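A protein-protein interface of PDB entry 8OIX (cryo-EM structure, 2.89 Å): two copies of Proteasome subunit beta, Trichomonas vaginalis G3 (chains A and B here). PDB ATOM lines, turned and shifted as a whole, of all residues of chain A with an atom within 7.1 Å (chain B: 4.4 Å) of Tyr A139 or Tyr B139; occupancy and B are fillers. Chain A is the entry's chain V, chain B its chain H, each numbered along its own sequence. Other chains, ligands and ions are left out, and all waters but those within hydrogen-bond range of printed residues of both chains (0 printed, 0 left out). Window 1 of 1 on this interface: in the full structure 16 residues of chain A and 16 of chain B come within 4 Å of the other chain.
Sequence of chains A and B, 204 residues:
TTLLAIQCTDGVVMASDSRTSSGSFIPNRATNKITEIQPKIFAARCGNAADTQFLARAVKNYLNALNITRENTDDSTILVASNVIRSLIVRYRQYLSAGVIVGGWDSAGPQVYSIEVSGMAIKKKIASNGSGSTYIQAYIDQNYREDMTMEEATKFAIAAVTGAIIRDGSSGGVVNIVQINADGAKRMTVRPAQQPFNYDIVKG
Ile A136 touches Ala B138, and with the chains exchanged Ala A138 touches Ile B136. Ala A138 touches Tyr B139, and with the chains exchanged Tyr A139 touches Ala B138. Tyr A139 touches its own counterpart, Tyr B139. Tyr A139 touches Gln B142, and with the chains exchanged Gln A142 touches Tyr B139. 12 positions are printed for both chains.
Printed residues of chain B that touch a printed residue of chain A: Ile B136, Gln B137, Ala B138, Tyr B139, Gln B142 and Phe B197. Of the 22 printed residues of chain A, 6 touch a printed residue of chain B. Among the printed residues, no Asp or Glu carboxylate lies within 4 Å of a Lys or Arg side-chain nitrogen of the other chain.
The backbone carbonyl oxygen of Tyr B139 sits close to the side-chain amide oxygen of Asn B143, at 2.8 Å. The backbone carbonyl oxygen (O) of Tyr A139 sits close to the side-chain amide oxygen (OD1) of Asn A143 (2.8 Å).
The backbone NH (N) of Ala B138 lies within hydrogen-bond range of the backbone carbonyl oxygen (O) of Tyr A135, at 3.0 Å.
Gln B137 touches Tyr A135 (N to O, 3.8 Å). Ala B138 touches Ile A136. CB of Ala A138 touches CG2 of Ile B136 (3.5 Å). Ala A138 touches Tyr B139 (CB to CB, 3.8 Å). CB of Tyr A139 touches CB of Ala B138, 3.8 Å away. CB of Tyr B139 touches N of Tyr A139, at 3.9 Å. Tyr A139 touches Gln B142 (CE1 to CG, 3.5 Å). Gln A142 touches Tyr B139 (CG to CE1, 3.5 Å). Gln A142 touches Phe B197. OE1 of Gln B142 touches CZ of Phe A197 (3.5 Å).
Of the printed residues of chain B, Ala A138 touches Ile B136 (3.5 Å) and Tyr B139 (3.8 Å). Of chain B, only Ala B138 (3.8 Å), Tyr B139 (3.9 Å) and Gln B142 (3.5 Å) come within 4 Å of Tyr A139. Of the printed residues of chain B, Gln A142 touches Tyr B139 and Phe B197. Tyr B139 touches just these residues of chain A: Ala A138 (3.8 Å), Tyr A139 (3.9 Å) and Gln A142 (3.5 Å). The nearest printed residue of chain B that does not touch Tyr A139 is Asn B143 (5.3 Å). The nearest printed residue of chain B that does not touch Tyr A135 is Ile B136 (4.4 Å).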
ATOM      1  N   LEU A   4       9.915  25.820  14.672  1.00  0.00           N
ATOM      2  CA  LEU A   4      10.577  26.596  13.624  1.00  0.00           C
ATOM      3  C   LEU A   4      11.431  27.673  14.286  1.00  0.00           C
ATOM      4  O   LEU A   4      10.922  28.738  14.639  1.00  0.00           O
ATOM      5  CB  LEU A   4       9.551  27.205  12.681  1.00  0.00           C
ATOM      6  CG  LEU A   4      10.154  27.986  11.521  1.00  0.00           C
ATOM      7  CD1 LEU A   4      11.007  27.056  10.691  1.00  0.00           C
ATOM      8  CD2 LEU A   4       9.067  28.624  10.681  1.00  0.00           C
ATOM      9  N   THR A 134       6.822  19.260   8.366  1.00  0.00           N
ATOM     10  CA  THR A 134       6.796  18.644   7.047  1.00  0.00           C
ATOM     11  C   THR A 134       5.906  19.438   6.106  1.00  0.00           C
ATOM     12  O   THR A 134       6.316  19.791   4.997  1.00  0.00           O
ATOM     13  CB  THR A 134       6.312  17.197   7.150  1.00  0.00           C
ATOM     14  OG1 THR A 134       4.983  17.175   7.681  1.00  0.00           O
ATOM     15  CG2 THR A 134       7.222  16.399   8.068  1.00  0.00           C
ATOM     16  N   TYR A 135       4.689  19.758   6.550  1.00  0.00           N
ATOM     17  CA  TYR A 135       3.747  20.468   5.697  1.00  0.00           C
ATOM     18  C   TYR A 135       4.256  21.838   5.279  1.00  0.00           C
ATOM     19  O   TYR A 135       3.823  22.356   4.245  1.00  0.00           O
ATOM     20  CB  TYR A 135       2.400  20.608   6.403  1.00  0.00           C
ATOM     21  CG  TYR A 135       1.811  19.286   6.829  1.00  0.00           C
ATOM     22  CD1 TYR A 135       1.224  18.438   5.903  1.00  0.00           C
ATOM     23  CD2 TYR A 135       1.853  18.880   8.153  1.00  0.00           C
ATOM     24  CE1 TYR A 135       0.692  17.227   6.285  1.00  0.00           C
ATOM     25  CE2 TYR A 135       1.323  17.670   8.542  1.00  0.00           C
ATOM     26  CZ  TYR A 135       0.742  16.850   7.606  1.00  0.00           C
ATOM     27  OH  TYR A 135       0.212  15.643   7.995  1.00  0.00           O
ATOM     28  N   ILE A 136       5.171  22.432   6.041  1.00  0.00           N
ATOM     29  CA  ILE A 136       5.650  23.776   5.761  1.00  0.00           C
ATOM     30  C   ILE A 136       7.088  23.781   5.268  1.00  0.00           C
ATOM     31  O   ILE A 136       7.698  24.846   5.192  1.00  0.00           O
ATOM     32  CB  ILE A 136       5.505  24.690   6.985  1.00  0.00           C
ATOM     33  CG1 ILE A 136       6.225  24.084   8.189  1.00  0.00           C
ATOM     34  CG2 ILE A 136       4.052  24.893   7.305  1.00  0.00           C
ATOM     35  CD1 ILE A 136       6.388  25.037   9.345  1.00  0.00           C
ATOM     36  N   GLN A 137       7.658  22.618   4.955  1.00  0.00           N
ATOM     37  CA  GLN A 137       9.030  22.606   4.449  1.00  0.00           C
ATOM     38  C   GLN A 137       9.162  23.430   3.170  1.00  0.00           C
ATOM     39  O   GLN A 137      10.029  24.307   3.070  1.00  0.00           O
ATOM     40  CB  GLN A 137       9.495  21.171   4.203  1.00  0.00           C
ATOM     41  CG  GLN A 137       9.769  20.372   5.464  1.00  0.00           C
ATOM     42  CD  GLN A 137      10.789  21.037   6.368  1.00  0.00           C
ATOM     43  OE1 GLN A 137      11.727  21.680   5.900  1.00  0.00           O
ATOM     44  NE2 GLN A 137      10.608  20.882   7.672  1.00  0.00           N
ATOM     45  N   ALA A 138       8.312  23.158   2.177  1.00  0.00           N
ATOM     46  CA  ALA A 138       8.349  23.929   0.936  1.00  0.00           C
ATOM     47  C   ALA A 138       8.024  25.398   1.177  1.00  0.00           C
ATOM     48  O   ALA A 138       8.629  26.282   0.559  1.00  0.00           O
ATOM     49  CB  ALA A 138       7.387  23.336  -0.086  1.00  0.00           C
ATOM     50  N   TYR A 139       7.049  25.676   2.043  1.00  0.00           N
ATOM     51  CA  TYR A 139       6.709  27.061   2.350  1.00  0.00           C
ATOM     52  C   TYR A 139       7.913  27.803   2.915  1.00  0.00           C
ATOM     53  O   TYR A 139       8.196  28.941   2.527  1.00  0.00           O
ATOM     54  CB  TYR A 139       5.539  27.115   3.333  1.00  0.00           C
ATOM     55  CG  TYR A 139       5.190  28.520   3.758  1.00  0.00           C
ATOM     56  CD1 TYR A 139       4.433  29.341   2.938  1.00  0.00           C
ATOM     57  CD2 TYR A 139       5.636  29.033   4.967  1.00  0.00           C
ATOM     58  CE1 TYR A 139       4.120  30.628   3.314  1.00  0.00           C
ATOM     59  CE2 TYR A 139       5.327  30.323   5.349  1.00  0.00           C
ATOM     60  CZ  TYR A 139       4.568  31.115   4.518  1.00  0.00           C
ATOM     61  OH  TYR A 139       4.252  32.399   4.887  1.00  0.00           O
ATOM     62  N   ILE A 140       8.626  27.171   3.848  1.00  0.00           N
ATOM     63  CA  ILE A 140       9.826  27.770   4.418  1.00  0.00           C
ATOM     64  C   ILE A 140      10.864  27.999   3.332  1.00  0.00           C
ATOM     65  O   ILE A 140      11.434  29.087   3.211  1.00  0.00           O
ATOM     66  CB  ILE A 140      10.381  26.879   5.544  1.00  0.00           C
ATOM     67  CG1 ILE A 140       9.445  26.902   6.750  1.00  0.00           C
ATOM     68  CG2 ILE A 140      11.776  27.324   5.937  1.00  0.00           C
ATOM     69  CD1 ILE A 140       9.674  25.759   7.700  1.00  0.00           C
ATOM     70  N   ASP A 141      11.103  26.980   2.503  1.00  0.00           N
ATOM     71  CA  ASP A 141      12.104  27.110   1.450  1.00  0.00           C
ATOM     72  C   ASP A 141      11.770  28.249   0.497  1.00  0.00           C
ATOM     73  O   ASP A 141      12.676  28.905  -0.029  1.00  0.00           O
ATOM     74  CB  ASP A 141      12.235  25.795   0.688  1.00  0.00           C
ATOM     75  CG  ASP A 141      12.690  24.654   1.572  1.00  0.00           C
ATOM     76  OD1 ASP A 141      13.533  24.891   2.462  1.00  0.00           O
ATOM     77  OD2 ASP A 141      12.208  23.520   1.375  1.00  0.00           O
ATOM     78  N   GLN A 142      10.483  28.502   0.267  1.00  0.00           N
ATOM     79  CA  GLN A 142      10.085  29.554  -0.660  1.00  0.00           C
ATOM     80  C   GLN A 142      10.075  30.926   0.004  1.00  0.00           C
ATOM     81  O   GLN A 142      10.316  31.936  -0.667  1.00  0.00           O
ATOM     82  CB  GLN A 142       8.707  29.228  -1.246  1.00  0.00           C
ATOM     83  CG  GLN A 142       7.959  30.401  -1.874  1.00  0.00           C
ATOM     84  CD  GLN A 142       8.717  31.044  -3.021  1.00  0.00           C
ATOM     85  OE1 GLN A 142       8.857  30.457  -4.093  1.00  0.00           O
ATOM     86  NE2 GLN A 142       9.208  32.258  -2.798  1.00  0.00           N
ATOM     87  N   ASN A 143       9.851  30.986   1.317  1.00  0.00           N
ATOM     88  CA  ASN A 143       9.673  32.256   2.005  1.00  0.00           C
ATOM     89  C   ASN A 143      10.781  32.597   2.992  1.00  0.00           C
ATOM     90  O   ASN A 143      10.788  33.716   3.516  1.00  0.00           O
ATOM     91  CB  ASN A 143       8.324  32.275   2.737  1.00  0.00           C
ATOM     92  CG  ASN A 143       7.148  32.165   1.791  1.00  0.00           C
ATOM     93  OD1 ASN A 143       6.667  31.070   1.506  1.00  0.00           O
ATOM     94  ND2 ASN A 143       6.679  33.303   1.296  1.00  0.00           N
ATOM     95  N   TYR A 144      11.709  31.685   3.266  1.00  0.00           N
ATOM     96  CA  TYR A 144      12.810  31.972   4.175  1.00  0.00           C
ATOM     97  C   TYR A 144      13.942  32.658   3.425  1.00  0.00           C
ATOM     98  O   TYR A 144      14.355  32.200   2.355  1.00  0.00           O
ATOM     99  CB  TYR A 144      13.337  30.702   4.842  1.00  0.00           C
ATOM    100  CG  TYR A 144      14.642  30.914   5.568  1.00  0.00           C
ATOM    101  CD1 TYR A 144      14.691  31.637   6.751  1.00  0.00           C
ATOM    102  CD2 TYR A 144      15.833  30.414   5.059  1.00  0.00           C
ATOM    103  CE1 TYR A 144      15.883  31.843   7.412  1.00  0.00           C
ATOM    104  CE2 TYR A 144      17.030  30.617   5.713  1.00  0.00           C
ATOM    105  CZ  TYR A 144      17.048  31.330   6.890  1.00  0.00           C
ATOM    106  OH  TYR A 144      18.237  31.534   7.548  1.00  0.00           O
ATOM    107  N   LYS A 155       7.389  37.371  11.705  1.00  0.00           N
ATOM    108  CA  LYS A 155       6.204  37.317  10.856  1.00  0.00           C
ATOM    109  C   LYS A 155       6.198  36.054  10.002  1.00  0.00           C
ATOM    110  O   LYS A 155       5.173  35.366   9.892  1.00  0.00           O
ATOM    111  CB  LYS A 155       6.135  38.563   9.974  1.00  0.00           C
ATOM    112  CG  LYS A 155       4.870  38.662   9.145  1.00  0.00           C
ATOM    113  CD  LYS A 155       4.893  39.891   8.254  1.00  0.00           C
ATOM    114  CE  LYS A 155       3.801  39.823   7.203  1.00  0.00           C
ATOM    115  NZ  LYS A 155       4.023  38.693   6.259  1.00  0.00           N
ATOM    116  N   PHE A 156       7.343  35.725   9.400  1.00  0.00           N
ATOM    117  CA  PHE A 156       7.419  34.533   8.562  1.00  0.00           C
ATOM    118  C   PHE A 156       7.196  33.266   9.377  1.00  0.00           C
ATOM    119  O   PHE A 156       6.548  32.326   8.909  1.00  0.00           O
ATOM    120  CB  PHE A 156       8.762  34.479   7.836  1.00  0.00           C
ATOM    121  CG  PHE A 156       9.183  33.094   7.443  1.00  0.00           C
ATOM    122  CD1 PHE A 156       8.640  32.479   6.331  1.00  0.00           C
ATOM    123  CD2 PHE A 156      10.133  32.411   8.178  1.00  0.00           C
ATOM    124  CE1 PHE A 156       9.027  31.205   5.972  1.00  0.00           C
ATOM    125  CE2 PHE A 156      10.524  31.140   7.822  1.00  0.00           C
ATOM    126  CZ  PHE A 156       9.972  30.538   6.717  1.00  0.00           C
ATOM    127  N   ALA A 157       7.736  33.218  10.595  1.00  0.00           N
ATOM    128  CA  ALA A 157       7.564  32.049  11.446  1.00  0.00           C
ATOM    129  C   ALA A 157       6.124  31.915  11.913  1.00  0.00           C
ATOM    130  O   ALA A 157       5.598  30.801  11.992  1.00  0.00           O
ATOM    131  CB  ALA A 157       8.514  32.131  12.638  1.00  0.00           C
ATOM    132  N   ILE A 158       5.466  33.034  12.225  1.00  0.00           N
ATOM    133  CA  ILE A 158       4.045  32.984  12.550  1.00  0.00           C
ATOM    134  C   ILE A 158       3.261  32.432  11.372  1.00  0.00           C
ATOM    135  O   ILE A 158       2.406  31.556  11.534  1.00  0.00           O
ATOM    136  CB  ILE A 158       3.528  34.373  12.964  1.00  0.00           C
ATOM    137  CG1 ILE A 158       4.174  34.832  14.267  1.00  0.00           C
ATOM    138  CG2 ILE A 158       2.026  34.348  13.133  1.00  0.00           C
ATOM    139  CD1 ILE A 158       4.018  36.311  14.530  1.00  0.00           C
ATOM    140  N   ALA A 159       3.559  32.916  10.164  1.00  0.00           N
ATOM    141  CA  ALA A 159       2.850  32.439   8.979  1.00  0.00           C
ATOM    142  C   ALA A 159       3.091  30.952   8.741  1.00  0.00           C
ATOM    143  O   ALA A 159       2.153  30.202   8.446  1.00  0.00           O
ATOM    144  CB  ALA A 159       3.272  33.256   7.761  1.00  0.00           C
ATOM    145  N   ALA A 160       4.341  30.505   8.870  1.00  0.00           N
ATOM    146  CA  ALA A 160       4.663  29.106   8.602  1.00  0.00           C
ATOM    147  C   ALA A 160       4.053  28.186   9.651  1.00  0.00           C
ATOM    148  O   ALA A 160       3.481  27.144   9.314  1.00  0.00           O
ATOM    149  CB  ALA A 160       6.175  28.919   8.537  1.00  0.00           C
ATOM    150  N   VAL A 161       4.166  28.549  10.929  1.00  0.00           N
ATOM    151  CA  VAL A 161       3.580  27.718  11.971  1.00  0.00           C
ATOM    152  C   VAL A 161       2.064  27.752  11.884  1.00  0.00           C
ATOM    153  O   VAL A 161       1.402  26.765  12.208  1.00  0.00           O
ATOM    154  CB  VAL A 161       4.100  28.156  13.352  1.00  0.00           C
ATOM    155  CG1 VAL A 161       3.349  27.448  14.464  1.00  0.00           C
ATOM    156  CG2 VAL A 161       5.576  27.849  13.453  1.00  0.00           C
ATOM    157  N   GLY A 163       0.395  27.940   8.965  1.00  0.00           N
ATOM    158  CA  GLY A 163       0.118  26.996   7.896  1.00  0.00           C
ATOM    159  C   GLY A 163       0.225  25.555   8.356  1.00  0.00           C
ATOM    160  O   GLY A 163      -0.608  24.715   8.006  1.00  0.00           O
ATOM    161  N   PRO A 196      -2.173  34.855  10.823  1.00  0.00           N
ATOM    162  CA  PRO A 196      -2.372  35.471   9.503  1.00  0.00           C
ATOM    163  C   PRO A 196      -3.292  34.678   8.594  1.00  0.00           C
ATOM    164  O   PRO A 196      -3.999  35.277   7.776  1.00  0.00           O
ATOM    165  CB  PRO A 196      -0.944  35.539   8.947  1.00  0.00           C
ATOM    166  CG  PRO A 196      -0.290  34.353   9.566  1.00  0.00           C
ATOM    167  CD  PRO A 196      -0.790  34.378  10.985  1.00  0.00           C
ATOM    168  N   PHE A 197      -3.305  33.356   8.709  1.00  0.00           N
ATOM    169  CA  PHE A 197      -4.083  32.491   7.838  1.00  0.00           C
ATOM    170  C   PHE A 197      -5.129  31.753   8.663  1.00  0.00           C
ATOM    171  O   PHE A 197      -5.095  31.745   9.896  1.00  0.00           O
ATOM    172  CB  PHE A 197      -3.191  31.475   7.111  1.00  0.00           C
ATOM    173  CG  PHE A 197      -1.915  32.052   6.563  1.00  0.00           C
ATOM    174  CD1 PHE A 197      -1.882  33.319   6.003  1.00  0.00           C
ATOM    175  CD2 PHE A 197      -0.738  31.327   6.630  1.00  0.00           C
ATOM    176  CE1 PHE A 197      -0.704  33.844   5.507  1.00  0.00           C
ATOM    177  CE2 PHE A 197       0.443  31.846   6.137  1.00  0.00           C
ATOM    178  CZ  PHE A 197       0.460  33.107   5.575  1.00  0.00           C
ATOM    179  N   ILE B 136       4.512  20.209   0.470  1.00  0.00           N
ATOM    180  CA  ILE B 136       4.088  21.390  -0.264  1.00  0.00           C
ATOM    181  C   ILE B 136       2.659  21.788   0.067  1.00  0.00           C
ATOM    182  O   ILE B 136       2.089  22.630  -0.622  1.00  0.00           O
ATOM    183  CB  ILE B 136       4.249  21.197  -1.778  1.00  0.00           C
ATOM    184  CG1 ILE B 136       3.488  19.954  -2.238  1.00  0.00           C
ATOM    185  CG2 ILE B 136       5.703  21.069  -2.128  1.00  0.00           C
ATOM    186  CD1 ILE B 136       3.344  19.849  -3.735  1.00  0.00           C
ATOM    187  N   GLN B 137       2.050  21.187   1.091  1.00  0.00           N
ATOM    188  CA  GLN B 137       0.687  21.578   1.443  1.00  0.00           C
ATOM    189  C   GLN B 137       0.604  23.062   1.795  1.00  0.00           C
ATOM    190  O   GLN B 137      -0.228  23.796   1.247  1.00  0.00           O
ATOM    191  CB  GLN B 137       0.173  20.729   2.606  1.00  0.00           C
ATOM    192  CG  GLN B 137      -0.150  19.293   2.244  1.00  0.00           C
ATOM    193  CD  GLN B 137      -1.158  19.185   1.116  1.00  0.00           C
ATOM    194  OE1 GLN B 137      -2.064  20.007   0.995  1.00  0.00           O
ATOM    195  NE2 GLN B 137      -1.002  18.164   0.283  1.00  0.00           N
ATOM    196  N   ALA B 138       1.459  23.521   2.713  1.00  0.00           N
ATOM    197  CA  ALA B 138       1.469  24.937   3.075  1.00  0.00           C
ATOM    198  C   ALA B 138       1.844  25.818   1.891  1.00  0.00           C
ATOM    199  O   ALA B 138       1.282  26.905   1.716  1.00  0.00           O
ATOM    200  CB  ALA B 138       2.424  25.180   4.239  1.00  0.00           C
ATOM    201  N   TYR B 139       2.816  25.383   1.087  1.00  0.00           N
ATOM    202  CA  TYR B 139       3.203  26.158  -0.088  1.00  0.00           C
ATOM    203  C   TYR B 139       2.018  26.346  -1.026  1.00  0.00           C
ATOM    204  O   TYR B 139       1.783  27.447  -1.538  1.00  0.00           O
ATOM    205  CB  TYR B 139       4.359  25.473  -0.817  1.00  0.00           C
ATOM    206  CG  TYR B 139       4.753  26.179  -2.090  1.00  0.00           C
ATOM    207  CD1 TYR B 139       5.552  27.312  -2.053  1.00  0.00           C
ATOM    208  CD2 TYR B 139       4.309  25.731  -3.325  1.00  0.00           C
ATOM    209  CE1 TYR B 139       5.908  27.969  -3.210  1.00  0.00           C
ATOM    210  CE2 TYR B 139       4.660  26.387  -4.488  1.00  0.00           C
ATOM    211  CZ  TYR B 139       5.461  27.504  -4.423  1.00  0.00           C
ATOM    212  OH  TYR B 139       5.819  28.164  -5.574  1.00  0.00           O
ATOM    213  N   ILE B 140       1.268  25.272  -1.274  1.00  0.00           N
ATOM    214  CA  ILE B 140       0.083  25.355  -2.118  1.00  0.00           C
ATOM    215  C   ILE B 140      -0.930  26.310  -1.506  1.00  0.00           C
ATOM    216  O   ILE B 140      -1.457  27.199  -2.180  1.00  0.00           O
ATOM    217  CB  ILE B 140      -0.521  23.954  -2.322  1.00  0.00           C
ATOM    218  CG1 ILE B 140       0.397  23.102  -3.196  1.00  0.00           C
ATOM    219  CG2 ILE B 140      -1.904  24.055  -2.934  1.00  0.00           C
ATOM    220  CD1 ILE B 140       0.110  21.629  -3.095  1.00  0.00           C
ATOM    221  N   ASP B 141      -1.193  26.156  -0.207  1.00  0.00           N
ATOM    222  CA  ASP B 141      -2.173  27.015   0.449  1.00  0.00           C
ATOM    223  C   ASP B 141      -1.783  28.483   0.355  1.00  0.00           C
ATOM    224  O   ASP B 141      -2.657  29.354   0.267  1.00  0.00           O
ATOM    225  CB  ASP B 141      -2.341  26.598   1.907  1.00  0.00           C
ATOM    226  CG  ASP B 141      -2.852  25.181   2.051  1.00  0.00           C
ATOM    227  OD1 ASP B 141      -3.698  24.767   1.231  1.00  0.00           O
ATOM    228  OD2 ASP B 141      -2.409  24.481   2.983  1.00  0.00           O
ATOM    229  N   GLN B 142      -0.483  28.777   0.366  1.00  0.00           N
ATOM    230  CA  GLN B 142      -0.034  30.163   0.314  1.00  0.00           C
ATOM    231  C   GLN B 142       0.018  30.694  -1.114  1.00  0.00           C
ATOM    232  O   GLN B 142      -0.175  31.895  -1.332  1.00  0.00           O
ATOM    233  CB  GLN B 142       1.339  30.282   0.983  1.00  0.00           C
ATOM    234  CG  GLN B 142       2.140  31.535   0.637  1.00  0.00           C
ATOM    235  CD  GLN B 142       1.424  32.819   1.009  1.00  0.00           C
ATOM    236  OE1 GLN B 142       1.277  33.143   2.188  1.00  0.00           O
ATOM    237  NE2 GLN B 142       0.975  33.559   0.001  1.00  0.00           N
ATOM    238  N   ASN B 143       0.223  29.821  -2.101  1.00  0.00           N
ATOM    239  CA  ASN B 143       0.438  30.254  -3.474  1.00  0.00           C
ATOM    240  C   ASN B 143      -0.671  29.859  -4.439  1.00  0.00           C
ATOM    241  O   ASN B 143      -0.643  30.304  -5.591  1.00  0.00           O
ATOM    242  CB  ASN B 143       1.777  29.712  -3.996  1.00  0.00           C
ATOM    243  CG  ASN B 143       2.961  30.243  -3.218  1.00  0.00           C
ATOM    244  OD1 ASN B 143       3.407  29.632  -2.249  1.00  0.00           O
ATOM    245  ND2 ASN B 143       3.479  31.389  -3.641  1.00  0.00           N
ATOM    246  N   PHE B 156       2.785  27.557 -11.179  1.00  0.00           N
ATOM    247  CA  PHE B 156       2.678  27.279  -9.750  1.00  0.00           C
ATOM    248  C   PHE B 156       2.841  25.794  -9.460  1.00  0.00           C
ATOM    249  O   PHE B 156       3.460  25.415  -8.462  1.00  0.00           O
ATOM    250  CB  PHE B 156       1.344  27.793  -9.210  1.00  0.00           C
ATOM    251  CG  PHE B 156       0.879  27.080  -7.974  1.00  0.00           C
ATOM    252  CD1 PHE B 156       1.415  27.386  -6.736  1.00  0.00           C
ATOM    253  CD2 PHE B 156      -0.107  26.115  -8.047  1.00  0.00           C
ATOM    254  CE1 PHE B 156       0.986  26.730  -5.602  1.00  0.00           C
ATOM    255  CE2 PHE B 156      -0.539  25.458  -6.916  1.00  0.00           C
ATOM    256  CZ  PHE B 156       0.006  25.767  -5.694  1.00  0.00           C
ATOM    257  N   ALA B 159       6.450  24.863  -9.731  1.00  0.00           N
ATOM    258  CA  ALA B 159       7.158  25.311  -8.536  1.00  0.00           C
ATOM    259  C   ALA B 159       6.867  24.412  -7.339  1.00  0.00           C
ATOM    260  O   ALA B 159       7.780  24.040  -6.594  1.00  0.00           O
ATOM    261  CB  ALA B 159       6.786  26.759  -8.226  1.00  0.00           C
ATOM    262  N   ALA B 160       5.599  24.047  -7.141  1.00  0.00           N
ATOM    263  CA  ALA B 160       5.231  23.234  -5.986  1.00  0.00           C
ATOM    264  C   ALA B 160       5.789  21.823  -6.099  1.00  0.00           C
ATOM    265  O   ALA B 160       6.327  21.282  -5.127  1.00  0.00           O
ATOM    266  CB  ALA B 160       3.712  23.200  -5.832  1.00  0.00           C
ATOM    267  N   PHE B 197      13.347  25.931  -8.882  1.00  0.00           N
ATOM    268  CA  PHE B 197      14.107  25.881  -7.645  1.00  0.00           C
ATOM    269  C   PHE B 197      15.111  24.740  -7.716  1.00  0.00           C
ATOM    270  O   PHE B 197      15.058  23.882  -8.599  1.00  0.00           O
ATOM    271  CB  PHE B 197      13.187  25.684  -6.429  1.00  0.00           C
ATOM    272  CG  PHE B 197      11.941  26.526  -6.452  1.00  0.00           C
ATOM    273  CD1 PHE B 197      11.965  27.829  -6.924  1.00  0.00           C
ATOM    274  CD2 PHE B 197      10.738  26.000  -6.017  1.00  0.00           C
ATOM    275  CE1 PHE B 197      10.813  28.594  -6.947  1.00  0.00           C
ATOM    276  CE2 PHE B 197       9.585  26.759  -6.038  1.00  0.00           C
ATOM    277  CZ  PHE B 197       9.622  28.058  -6.503  1.00  0.00           C
